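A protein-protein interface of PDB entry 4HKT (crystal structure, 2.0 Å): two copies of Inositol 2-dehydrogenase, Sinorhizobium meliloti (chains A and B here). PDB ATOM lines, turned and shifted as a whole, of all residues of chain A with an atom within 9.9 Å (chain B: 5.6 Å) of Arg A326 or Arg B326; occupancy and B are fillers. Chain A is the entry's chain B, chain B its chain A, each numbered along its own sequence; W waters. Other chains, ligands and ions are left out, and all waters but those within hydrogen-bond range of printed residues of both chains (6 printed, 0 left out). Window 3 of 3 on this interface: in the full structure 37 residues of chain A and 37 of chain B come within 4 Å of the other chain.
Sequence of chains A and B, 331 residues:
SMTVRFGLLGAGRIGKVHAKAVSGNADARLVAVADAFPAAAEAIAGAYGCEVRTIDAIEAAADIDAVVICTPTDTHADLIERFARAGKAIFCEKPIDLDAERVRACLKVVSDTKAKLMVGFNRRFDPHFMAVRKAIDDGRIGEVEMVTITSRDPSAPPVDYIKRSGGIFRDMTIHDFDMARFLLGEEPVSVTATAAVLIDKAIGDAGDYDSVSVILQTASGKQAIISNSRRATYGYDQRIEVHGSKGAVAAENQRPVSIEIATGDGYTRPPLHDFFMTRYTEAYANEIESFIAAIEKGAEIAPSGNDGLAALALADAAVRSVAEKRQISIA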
ATOM      1  N   SER A 190       4.181  -6.887  -7.652  1.00  0.00           N
ATOM      2  CA  SER A 190       5.334  -7.716  -7.481  1.00  0.00           C
ATOM      3  C   SER A 190       5.607  -8.575  -8.721  1.00  0.00           C
ATOM      4  O   SER A 190       4.695  -9.037  -9.410  1.00  0.00           O
ATOM      5  CB  SER A 190       5.208  -8.610  -6.242  1.00  0.00           C
ATOM      6  OG  SER A 190       4.272  -9.656  -6.457  1.00  0.00           O
ATOM      7  N   VAL A 191       6.890  -8.773  -8.978  1.00  0.00           N
ATOM      8  CA  VAL A 191       7.364  -9.587 -10.096  1.00  0.00           C
ATOM      9  C   VAL A 191       8.412 -10.582  -9.622  1.00  0.00           C
ATOM     10  O   VAL A 191       9.332 -10.208  -8.924  1.00  0.00           O
ATOM     11  CB  VAL A 191       7.990  -8.706 -11.159  1.00  0.00           C
ATOM     12  CG1 VAL A 191       8.479  -9.555 -12.328  1.00  0.00           C
ATOM     13  CG2 VAL A 191       6.968  -7.710 -11.643  1.00  0.00           C
ATOM     14  N   THR A 192       8.255 -11.840  -9.981  1.00  0.00           N
ATOM     15  CA  THR A 192       9.324 -12.784  -9.760  1.00  0.00           C
ATOM     16  C   THR A 192       9.526 -13.582 -11.042  1.00  0.00           C
ATOM     17  O   THR A 192       8.556 -13.921 -11.761  1.00  0.00           O
ATOM     18  CB  THR A 192       9.080 -13.634  -8.481  1.00  0.00           C
ATOM     19  OG1 THR A 192      10.318 -14.263  -8.080  1.00  0.00           O
ATOM     20  CG2 THR A 192       8.017 -14.639  -8.712  1.00  0.00           C
ATOM     21  N   ALA A 193      10.786 -13.823 -11.372  1.00  0.00           N
ATOM     22  CA  ALA A 193      11.119 -14.347 -12.694  1.00  0.00           C
ATOM     23  C   ALA A 193      12.316 -15.263 -12.681  1.00  0.00           C
ATOM     24  O   ALA A 193      13.173 -15.185 -11.799  1.00  0.00           O
ATOM     25  CB  ALA A 193      11.426 -13.209 -13.635  1.00  0.00           C
ATOM     26  N   THR A 194      12.332 -16.161 -13.651  1.00  0.00           N
ATOM     27  CA  THR A 194      13.492 -17.011 -13.876  1.00  0.00           C
ATOM     28  C   THR A 194      13.839 -16.924 -15.346  1.00  0.00           C
ATOM     29  O   THR A 194      12.992 -16.605 -16.175  1.00  0.00           O
ATOM     30  CB  THR A 194      13.208 -18.466 -13.522  1.00  0.00           C
ATOM     31  OG1 THR A 194      12.073 -18.908 -14.258  1.00  0.00           O
ATOM     32  CG2 THR A 194      12.950 -18.627 -12.005  1.00  0.00           C
ATOM     33  N   SER A 213      10.295 -17.369 -17.466  1.00  0.00           N
ATOM     34  CA  SER A 213       9.056 -17.632 -16.768  1.00  0.00           C
ATOM     35  C   SER A 213       8.897 -16.498 -15.745  1.00  0.00           C
ATOM     36  O   SER A 213       9.866 -16.102 -15.083  1.00  0.00           O
ATOM     37  CB  SER A 213       9.130 -18.941 -16.028  1.00  0.00           C
ATOM     38  OG  SER A 213       9.441 -20.034 -16.844  1.00  0.00           O
ATOM     39  N   VAL A 214       7.685 -15.950 -15.646  1.00  0.00           N
ATOM     40  CA  VAL A 214       7.424 -14.818 -14.739  1.00  0.00           C
ATOM     41  C   VAL A 214       6.114 -15.034 -13.979  1.00  0.00           C
ATOM     42  O   VAL A 214       5.206 -15.578 -14.522  1.00  0.00           O
ATOM     43  CB  VAL A 214       7.329 -13.499 -15.492  1.00  0.00           C
ATOM     44  CG1 VAL A 214       7.256 -12.344 -14.506  1.00  0.00           C
ATOM     45  CG2 VAL A 214       8.523 -13.278 -16.398  1.00  0.00           C
ATOM     46  N   ILE A 215       6.073 -14.665 -12.712  1.00  0.00           N
ATOM     47  CA  ILE A 215       4.844 -14.564 -11.951  1.00  0.00           C
ATOM     48  C   ILE A 215       4.676 -13.120 -11.476  1.00  0.00           C
ATOM     49  O   ILE A 215       5.574 -12.562 -10.821  1.00  0.00           O
ATOM     50  CB  ILE A 215       4.818 -15.452 -10.693  1.00  0.00           C
ATOM     51  CG1 ILE A 215       5.123 -16.898 -10.998  1.00  0.00           C
ATOM     52  CG2 ILE A 215       3.445 -15.332 -10.020  1.00  0.00           C
ATOM     53  CD1 ILE A 215       5.520 -17.687  -9.739  1.00  0.00           C
ATOM     54  N   ASP A 316      11.607  -4.232 -16.240  1.00  0.00           N
ATOM     55  CA  ASP A 316      12.800  -3.846 -15.445  1.00  0.00           C
ATOM     56  C   ASP A 316      12.843  -4.651 -14.113  1.00  0.00           C
ATOM     57  O   ASP A 316      13.922  -5.126 -13.684  1.00  0.00           O
ATOM     58  CB  ASP A 316      12.797  -2.347 -15.126  1.00  0.00           C
ATOM     59  CG  ASP A 316      13.114  -1.458 -16.330  1.00  0.00           C
ATOM     60  OD1 ASP A 316      13.732  -1.903 -17.322  1.00  0.00           O
ATOM     61  OD2 ASP A 316      12.726  -0.276 -16.278  1.00  0.00           O
ATOM     62  N   ALA A 317      11.666  -4.774 -13.476  1.00  0.00           N
ATOM     63  CA  ALA A 317      11.524  -5.581 -12.291  1.00  0.00           C
ATOM     64  C   ALA A 317      11.840  -7.041 -12.575  1.00  0.00           C
ATOM     65  O   ALA A 317      12.507  -7.664 -11.760  1.00  0.00           O
ATOM     66  CB  ALA A 317      10.134  -5.425 -11.657  1.00  0.00           C
ATOM     67  N   ALA A 318      11.380  -7.591 -13.711  1.00  0.00           N
ATOM     68  CA  ALA A 318      11.763  -8.961 -14.071  1.00  0.00           C
ATOM     69  C   ALA A 318      13.267  -9.183 -14.198  1.00  0.00           C
ATOM     70  O   ALA A 318      13.757 -10.203 -13.759  1.00  0.00           O
ATOM     71  CB  ALA A 318      11.049  -9.470 -15.338  1.00  0.00           C
ATOM     72  N   VAL A 319      13.979  -8.237 -14.795  1.00  0.00           N
ATOM     73  CA  VAL A 319      15.422  -8.315 -14.970  1.00  0.00           C
ATOM     74  C   VAL A 319      16.117  -8.385 -13.599  1.00  0.00           C
ATOM     75  O   VAL A 319      16.979  -9.244 -13.399  1.00  0.00           O
ATOM     76  CB  VAL A 319      15.934  -7.091 -15.784  1.00  0.00           C
ATOM     77  CG1 VAL A 319      17.450  -7.053 -15.914  1.00  0.00           C
ATOM     78  CG2 VAL A 319      15.353  -7.065 -17.222  1.00  0.00           C
ATOM     79  N   ARG A 320      15.735  -7.491 -12.689  1.00  0.00           N
ATOM     80  CA  ARG A 320      16.257  -7.462 -11.305  1.00  0.00           C
ATOM     81  C   ARG A 320      15.928  -8.723 -10.556  1.00  0.00           C
ATOM     82  O   ARG A 320      16.780  -9.259  -9.852  1.00  0.00           O
ATOM     83  CB  ARG A 320      15.716  -6.266 -10.509  1.00  0.00           C
ATOM     84  CG  ARG A 320      16.275  -4.895 -10.879  1.00  0.00           C
ATOM     85  CD  ARG A 320      15.824  -3.826  -9.877  1.00  0.00           C
ATOM     86  NE  ARG A 320      16.161  -4.192  -8.489  1.00  0.00           N
ATOM     87  CZ  ARG A 320      15.595  -3.701  -7.386  1.00  0.00           C
ATOM     88  NH1 ARG A 320      14.592  -2.825  -7.425  1.00  0.00           N
ATOM     89  NH2 ARG A 320      16.015  -4.133  -6.209  1.00  0.00           N
ATOM     90  N   SER A 321      14.718  -9.236 -10.734  1.00  0.00           N
ATOM     91  CA  SER A 321      14.303 -10.434 -10.046  1.00  0.00           C
ATOM     92  C   SER A 321      15.207 -11.636 -10.422  1.00  0.00           C
ATOM     93  O   SER A 321      15.639 -12.399  -9.537  1.00  0.00           O
ATOM     94  CB  SER A 321      12.872 -10.802 -10.394  1.00  0.00           C
ATOM     95  OG  SER A 321      12.541 -12.015  -9.741  1.00  0.00           O
ATOM     96  N   VAL A 322      15.503 -11.784 -11.720  1.00  0.00           N
ATOM     97  CA  VAL A 322      16.355 -12.854 -12.144  1.00  0.00           C
ATOM     98  C   VAL A 322      17.743 -12.662 -11.535  1.00  0.00           C
ATOM     99  O   VAL A 322      18.307 -13.609 -11.004  1.00  0.00           O
ATOM    100  CB  VAL A 322      16.496 -12.953 -13.652  1.00  0.00           C
ATOM    101  CG1 VAL A 322      17.564 -13.987 -13.988  1.00  0.00           C
ATOM    102  CG2 VAL A 322      15.187 -13.357 -14.322  1.00  0.00           C
ATOM    103  N   ALA A 323      18.277 -11.445 -11.599  1.00  0.00           N
ATOM    104  CA  ALA A 323      19.634 -11.190 -11.096  1.00  0.00           C
ATOM    105  C   ALA A 323      19.760 -11.338  -9.590  1.00  0.00           C
ATOM    106  O   ALA A 323      20.756 -11.848  -9.132  1.00  0.00           O
ATOM    107  CB  ALA A 323      20.106  -9.830 -11.520  1.00  0.00           C
ATOM    108  N   GLU A 324      18.744 -10.914  -8.835  1.00  0.00           N
ATOM    109  CA  GLU A 324      18.796 -10.885  -7.377  1.00  0.00           C
ATOM    110  C   GLU A 324      18.158 -12.113  -6.738  1.00  0.00           C
ATOM    111  O   GLU A 324      18.226 -12.275  -5.549  1.00  0.00           O
ATOM    112  CB  GLU A 324      18.101  -9.618  -6.862  1.00  0.00           C
ATOM    113  CG  GLU A 324      18.858  -8.360  -7.235  1.00  0.00           C
ATOM    114  CD  GLU A 324      18.153  -7.056  -6.895  1.00  0.00           C
ATOM    115  OE1 GLU A 324      17.349  -7.003  -5.943  1.00  0.00           O
ATOM    116  OE2 GLU A 324      18.421  -6.062  -7.603  1.00  0.00           O
ATOM    117  N   LYS A 325      17.555 -12.972  -7.545  1.00  0.00           N
ATOM    118  CA  LYS A 325      16.899 -14.190  -7.091  1.00  0.00           C
ATOM    119  C   LYS A 325      15.783 -13.938  -6.061  1.00  0.00           C
ATOM    120  O   LYS A 325      15.584 -14.731  -5.142  1.00  0.00           O
ATOM    121  CB  LYS A 325      17.954 -15.169  -6.536  1.00  0.00           C
ATOM    122  CG  LYS A 325      18.980 -15.583  -7.572  1.00  0.00           C
ATOM    123  CD  LYS A 325      19.796 -16.748  -7.045  1.00  0.00           C
ATOM    124  CE  LYS A 325      20.777 -17.242  -8.079  1.00  0.00           C
ATOM    125  NZ  LYS A 325      21.996 -16.408  -8.034  1.00  0.00           N
ATOM    126  N   ARG A 326      15.062 -12.839  -6.234  1.00  0.00           N
ATOM    127  CA  ARG A 326      13.963 -12.532  -5.362  1.00  0.00           C
ATOM    128  C   ARG A 326      12.853 -11.773  -6.073  1.00  0.00           C
ATOM    129  O   ARG A 326      13.025 -11.244  -7.172  1.00  0.00           O
ATOM    130  CB  ARG A 326      14.444 -11.750  -4.174  1.00  0.00           C
ATOM    131  CG  ARG A 326      15.167 -10.463  -4.478  1.00  0.00           C
ATOM    132  CD  ARG A 326      15.285  -9.598  -3.213  1.00  0.00           C
ATOM    133  NE  ARG A 326      15.978 -10.324  -2.151  1.00  0.00           N
ATOM    134  CZ  ARG A 326      15.442 -10.822  -1.024  1.00  0.00           C
ATOM    135  NH1 ARG A 326      14.151 -10.661  -0.709  1.00  0.00           N
ATOM    136  NH2 ARG A 326      16.228 -11.496  -0.191  1.00  0.00           N
ATOM    137  N   GLN A 327      11.738 -11.692  -5.379  1.00  0.00           N
ATOM    138  CA  GLN A 327      10.602 -10.968  -5.815  1.00  0.00           C
ATOM    139  C   GLN A 327      10.923  -9.457  -5.739  1.00  0.00           C
ATOM    140  O   GLN A 327      11.535  -9.006  -4.801  1.00  0.00           O
ATOM    141  CB  GLN A 327       9.442 -11.334  -4.899  1.00  0.00           C
ATOM    142  CG  GLN A 327       8.072 -11.183  -5.482  1.00  0.00           C
ATOM    143  CD  GLN A 327       7.005 -11.590  -4.460  1.00  0.00           C
ATOM    144  OE1 GLN A 327       6.486 -10.750  -3.768  1.00  0.00           O
ATOM    145  NE2 GLN A 327       6.800 -12.877  -4.281  1.00  0.00           N
ATOM    146  N   ILE A 328      10.549  -8.719  -6.769  1.00  0.00           N
ATOM    147  CA  ILE A 328      10.797  -7.295  -6.853  1.00  0.00           C
ATOM    148  C   ILE A 328       9.472  -6.563  -6.839  1.00  0.00           C
ATOM    149  O   ILE A 328       8.587  -6.850  -7.645  1.00  0.00           O
ATOM    150  CB  ILE A 328      11.579  -6.906  -8.116  1.00  0.00           C
ATOM    151  CG1 ILE A 328      12.907  -7.647  -8.166  1.00  0.00           C
ATOM    152  CG2 ILE A 328      11.814  -5.375  -8.164  1.00  0.00           C
ATOM    153  CD1 ILE A 328      13.924  -7.252  -7.092  1.00  0.00           C
ATOM    154  N   SER A 329       9.334  -5.598  -5.940  1.00  0.00           N
ATOM    155  CA  SER A 329       8.068  -4.894  -5.801  1.00  0.00           C
ATOM    156  C   SER A 329       8.074  -3.705  -6.760  1.00  0.00           C
ATOM    157  O   SER A 329       9.127  -3.189  -7.113  1.00  0.00           O
ATOM    158  CB  SER A 329       7.832  -4.480  -4.340  1.00  0.00           C
ATOM    159  OG  SER A 329       8.917  -3.670  -3.952  1.00  0.00           O
ATOM    160  N   VAL B 191      13.164 -23.036  -6.387  1.00  0.00           N
ATOM    161  CA  VAL B 191      11.726 -22.906  -6.330  1.00  0.00           C
ATOM    162  C   VAL B 191      11.365 -21.458  -6.057  1.00  0.00           C
ATOM    163  O   VAL B 191      11.891 -20.844  -5.140  1.00  0.00           O
ATOM    164  CB  VAL B 191      11.170 -23.772  -5.192  1.00  0.00           C
ATOM    165  CG1 VAL B 191       9.689 -23.608  -5.076  1.00  0.00           C
ATOM    166  CG2 VAL B 191      11.531 -25.246  -5.403  1.00  0.00           C
ATOM    167  N   THR B 192      10.447 -20.892  -6.843  1.00  0.00           N
ATOM    168  CA  THR B 192       9.944 -19.520  -6.647  1.00  0.00           C
ATOM    169  C   THR B 192       8.432 -19.632  -6.664  1.00  0.00           C
ATOM    170  O   THR B 192       7.887 -20.240  -7.572  1.00  0.00           O
ATOM    171  CB  THR B 192      10.356 -18.581  -7.825  1.00  0.00           C
ATOM    172  OG1 THR B 192      11.775 -18.439  -7.868  1.00  0.00           O
ATOM    173  CG2 THR B 192       9.743 -17.203  -7.684  1.00  0.00           C
ATOM    174  N   ALA B 193       7.745 -19.069  -5.687  1.00  0.00           N
ATOM    175  CA  ALA B 193       6.308 -19.253  -5.619  1.00  0.00           C
ATOM    176  C   ALA B 193       5.566 -18.032  -5.108  1.00  0.00           C
ATOM    177  O   ALA B 193       6.118 -17.247  -4.365  1.00  0.00           O
ATOM    178  CB  ALA B 193       6.028 -20.428  -4.698  1.00  0.00           C
ATOM    179  N   ARG B 320       8.374 -21.615   1.973  1.00  0.00           N
ATOM    180  CA  ARG B 320       9.375 -20.661   2.366  1.00  0.00           C
ATOM    181  C   ARG B 320       9.556 -19.531   1.326  1.00  0.00           C
ATOM    182  O   ARG B 320       9.723 -18.361   1.678  1.00  0.00           O
ATOM    183  CB  ARG B 320      10.679 -21.413   2.579  1.00  0.00           C
ATOM    184  CG  ARG B 320      11.705 -20.605   3.284  1.00  0.00           C
ATOM    185  CD  ARG B 320      12.995 -21.358   3.432  1.00  0.00           C
ATOM    186  NE  ARG B 320      13.907 -20.577   4.222  1.00  0.00           N
ATOM    187  CZ  ARG B 320      15.222 -20.779   4.278  1.00  0.00           C
ATOM    188  NH1 ARG B 320      15.800 -21.723   3.545  1.00  0.00           N
ATOM    189  NH2 ARG B 320      15.967 -20.032   5.090  1.00  0.00           N
ATOM    190  N   SER B 321       9.444 -19.867   0.041  1.00  0.00           N
ATOM    191  CA  SER B 321       9.563 -18.859  -1.013  1.00  0.00           C
ATOM    192  C   SER B 321       8.432 -17.831  -0.917  1.00  0.00           C
ATOM    193  O   SER B 321       8.636 -16.638  -1.078  1.00  0.00           O
ATOM    194  CB  SER B 321       9.575 -19.512  -2.393  1.00  0.00           C
ATOM    195  OG  SER B 321       9.440 -18.516  -3.412  1.00  0.00           O
ATOM    196  N   VAL B 322       7.238 -18.305  -0.642  1.00  0.00           N
ATOM    197  CA  VAL B 322       6.091 -17.417  -0.472  1.00  0.00           C
ATOM    198  C   VAL B 322       6.318 -16.495   0.728  1.00  0.00           C
ATOM    199  O   VAL B 322       6.215 -15.256   0.592  1.00  0.00           O
ATOM    200  CB  VAL B 322       4.759 -18.170  -0.329  1.00  0.00           C
ATOM    201  CG1 VAL B 322       3.625 -17.205   0.024  1.00  0.00           C
ATOM    202  CG2 VAL B 322       4.376 -18.867  -1.619  1.00  0.00           C
ATOM    203  N   GLU B 324       9.215 -15.711   2.391  1.00  0.00           N
ATOM    204  CA  GLU B 324      10.360 -14.853   2.287  1.00  0.00           C
ATOM    205  C   GLU B 324      10.483 -14.063   0.976  1.00  0.00           C
ATOM    206  O   GLU B 324      11.468 -13.334   0.801  1.00  0.00           O
ATOM    207  CB  GLU B 324      11.622 -15.654   2.568  1.00  0.00           C
ATOM    208  CG  GLU B 324      11.501 -16.432   3.874  1.00  0.00           C
ATOM    209  CD  GLU B 324      12.798 -17.121   4.287  1.00  0.00           C
ATOM    210  OE1 GLU B 324      13.850 -16.785   3.729  1.00  0.00           O
ATOM    211  OE2 GLU B 324      12.759 -18.011   5.166  1.00  0.00           O
ATOM    212  N   LYS B 325       9.477 -14.174   0.099  1.00  0.00           N
ATOM    213  CA  LYS B 325       9.433 -13.374  -1.149  1.00  0.00           C
ATOM    214  C   LYS B 325      10.700 -13.527  -1.972  1.00  0.00           C
ATOM    215  O   LYS B 325      11.245 -12.543  -2.511  1.00  0.00           O
ATOM    216  CB  LYS B 325       9.195 -11.881  -0.847  1.00  0.00           C
ATOM    217  CG  LYS B 325       7.952 -11.607  -0.031  1.00  0.00           C
ATOM    218  CD  LYS B 325       7.977 -10.195   0.535  1.00  0.00           C
ATOM    219  CE  LYS B 325       6.892  -9.972   1.583  1.00  0.00           C
ATOM    220  NZ  LYS B 325       7.077 -10.705   2.881  1.00  0.00           N
ATOM    221  N   ARG B 326      11.169 -14.766  -2.100  1.00  0.00           N
ATOM    222  CA  ARG B 326      12.419 -15.030  -2.794  1.00  0.00           C
ATOM    223  C   ARG B 326      12.533 -16.465  -3.286  1.00  0.00           C
ATOM    224  O   ARG B 326      11.822 -17.359  -2.832  1.00  0.00           O
ATOM    225  CB  ARG B 326      13.635 -14.672  -1.925  1.00  0.00           C
ATOM    226  CG  ARG B 326      13.937 -15.626  -0.772  1.00  0.00           C
ATOM    227  CD  ARG B 326      15.057 -15.108   0.128  1.00  0.00           C
ATOM    228  NE  ARG B 326      15.293 -16.025   1.236  1.00  0.00           N
ATOM    229  CZ  ARG B 326      16.152 -17.061   1.225  1.00  0.00           C
ATOM    230  NH1 ARG B 326      16.903 -17.340   0.165  1.00  0.00           N
ATOM    231  NH2 ARG B 326      16.261 -17.835   2.296  1.00  0.00           N
ATOM    232  N   GLN B 327      13.467 -16.653  -4.214  1.00  0.00           N
ATOM    233  CA  GLN B 327      13.766 -17.950  -4.740  1.00  0.00           C
ATOM    234  C   GLN B 327      14.525 -18.747  -3.676  1.00  0.00           C
ATOM    235  O   GLN B 327      15.467 -18.240  -3.064  1.00  0.00           O
ATOM    236  CB  GLN B 327      14.614 -17.804  -6.021  1.00  0.00           C
ATOM    237  CG  GLN B 327      14.789 -19.091  -6.762  1.00  0.00           C
ATOM    238  CD  GLN B 327      15.712 -18.908  -7.959  1.00  0.00           C
ATOM    239  OE1 GLN B 327      15.256 -18.764  -9.074  1.00  0.00           O
ATOM    240  NE2 GLN B 327      17.000 -18.880  -7.715  1.00  0.00           N
ATOM    241  N   ILE B 328      14.092 -19.977  -3.438  1.00  0.00           N
ATOM    242  CA  ILE B 328      14.746 -20.868  -2.464  1.00  0.00           C
ATOM    243  C   ILE B 328      15.519 -21.968  -3.194  1.00  0.00           C
ATOM    244  O   ILE B 328      14.956 -22.731  -3.991  1.00  0.00           O
ATOM    245  CB  ILE B 328      13.689 -21.504  -1.514  1.00  0.00           C
ATOM    246  CG1 ILE B 328      12.942 -20.398  -0.722  1.00  0.00           C
ATOM    247  CG2 ILE B 328      14.322 -22.526  -0.558  1.00  0.00           C
ATOM    248  CD1 ILE B 328      13.831 -19.492   0.136  1.00  0.00           C
HETATM  249  O   HOH W   1      17.026 -16.472 -11.026  1.00  0.00           O
HETATM  250  O   HOH W   2      10.254 -15.089  -5.214  1.00  0.00           O
HETATM  251  O   HOH W   3       5.103 -14.003  -1.703  1.00  0.00           O
HETATM  252  O   HOH W   4       8.260 -15.689  -3.722  1.00  0.00           O
HETATM  253  O   HOH W   5      16.989 -16.058  -2.579  1.00  0.00           O
HETATM  254  O   HOH W   6      11.790  -9.995  -2.166  1.00  0.00           O
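The backbone carbonyl oxygen of Lys B325 is in hydrogen-bond range of the backbone NH of Gln A327 (3.0 Å). The backbone carbonyl oxygen (O) of Lys A325 sits at hydrogen-bond distance from the backbone NH (N) of Gln B327 (3.0 Å).
The side-chain hydroxyl (OG) of Ser B321 sits at hydrogen-bond distance from the backbone carbonyl oxygen (O) of Arg B326 (2.7 Å). NE of Arg B326 lies within salt-bridge range of OE1 of Glu B324 (3.0 Å). The backbone carbonyl oxygen of Thr A192 sits at hydrogen-bond distance from the backbone NH of Ile A215, 2.8 Å away. The backbone NH (N) of Thr A194 sits at hydrogen-bond distance from the backbone carbonyl oxygen (O) of Ser A213 (2.9 Å). O of Arg A326 lies within hydrogen-bond range of OG of Ser A321, at 2.7 Å.
Thr B192 touches Thr A192 (CG2 to OG1, 3.0 Å). Thr A194 touches Gln B327. O of Lys A325 touches CB of Arg B326 (3.8 Å). Arg A326 touches Lys B325. CB of Arg A326 touches CB of Arg B326, at 3.8 Å.
Of the printed residues of chain B, Thr A192 touches Thr B192. Ala A317 touches none of the printed residues of chain B. Of the printed residues of chain B, Lys A325 touches Arg B326 and Gln B327. Of the printed residues of chain B, Arg A326 touches Lys B325 (3.7 Å) and Arg B326 (3.8 Å). Of the printed residues of chain B, Gln A327 touches Lys B325 (3.0 Å). Of the printed residues of chain A, Thr B192 touches Thr A192. No residue of chain A comes within 4 Å of Ser B321. No residue of chain A comes within 4 Å of Glu B324. Arg B326 touches just these residues of chain A: Lys A325 (3.8 Å) and Arg A326 (3.8 Å). Of the printed residues of chain A, Gln B327 touches Thr A194 and Lys A325.
Of the 22 printed residues of chain A, 5 touch a printed residue of chain B. Among the printed residues, 7 pairs touch across the chains. Among the printed residues, no Asp or Glu carboxylate lies within 4 Å of a Lys or Arg side-chain nitrogen of the other chain.
Thr A192 touches its own counterpart, Thr B192. Lys A325 touches Arg B326, and with the chains exchanged Arg A326 touches Lys B325. Lys A325 touches Gln B327, and with the chains exchanged Gln A327 touches Lys B325. Arg B326 touches its own counterpart, Arg A326. Of the 7 pairs that touch across the chains among the printed residues, 6 have their exchanged pair printed and touching as well.
Water W6 lies within hydrogen-bond range of O of Lys B325 (2.6 Å), O of Gln A327 (2.8 Å) and NH1 of Arg A326 (2.9 Å). Water W5 lies within hydrogen-bond range of O of Gln B327 (2.7 Å), NH1 of Arg B326 (3.0 Å) and O of Lys A325 (3.2 Å). Water W4 lies within hydrogen-bond range of the backbone carbonyl oxygen of Ala B193 (2.7 Å), the backbone carbonyl oxygen of Ser B321 (2.8 Å), the side-chain amide nitrogen of Gln A327 (3.2 Å) and the backbone NH of Arg B326 (3.5 Å). Water W3 bridges O of Val B322 (2.8 Å) and NE2 of Gln A327 (3.3 Å). Water W2 bridges the side-chain hydroxyl of Thr A192 (3.0 Å) and the backbone NH of Arg B326 (3.3 Å). Water W1 bridges the backbone carbonyl oxygen (O) of Val A322 (3.1 Å) and the side-chain amide oxygen (OE1) of Gln B327 (3.5 Å).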
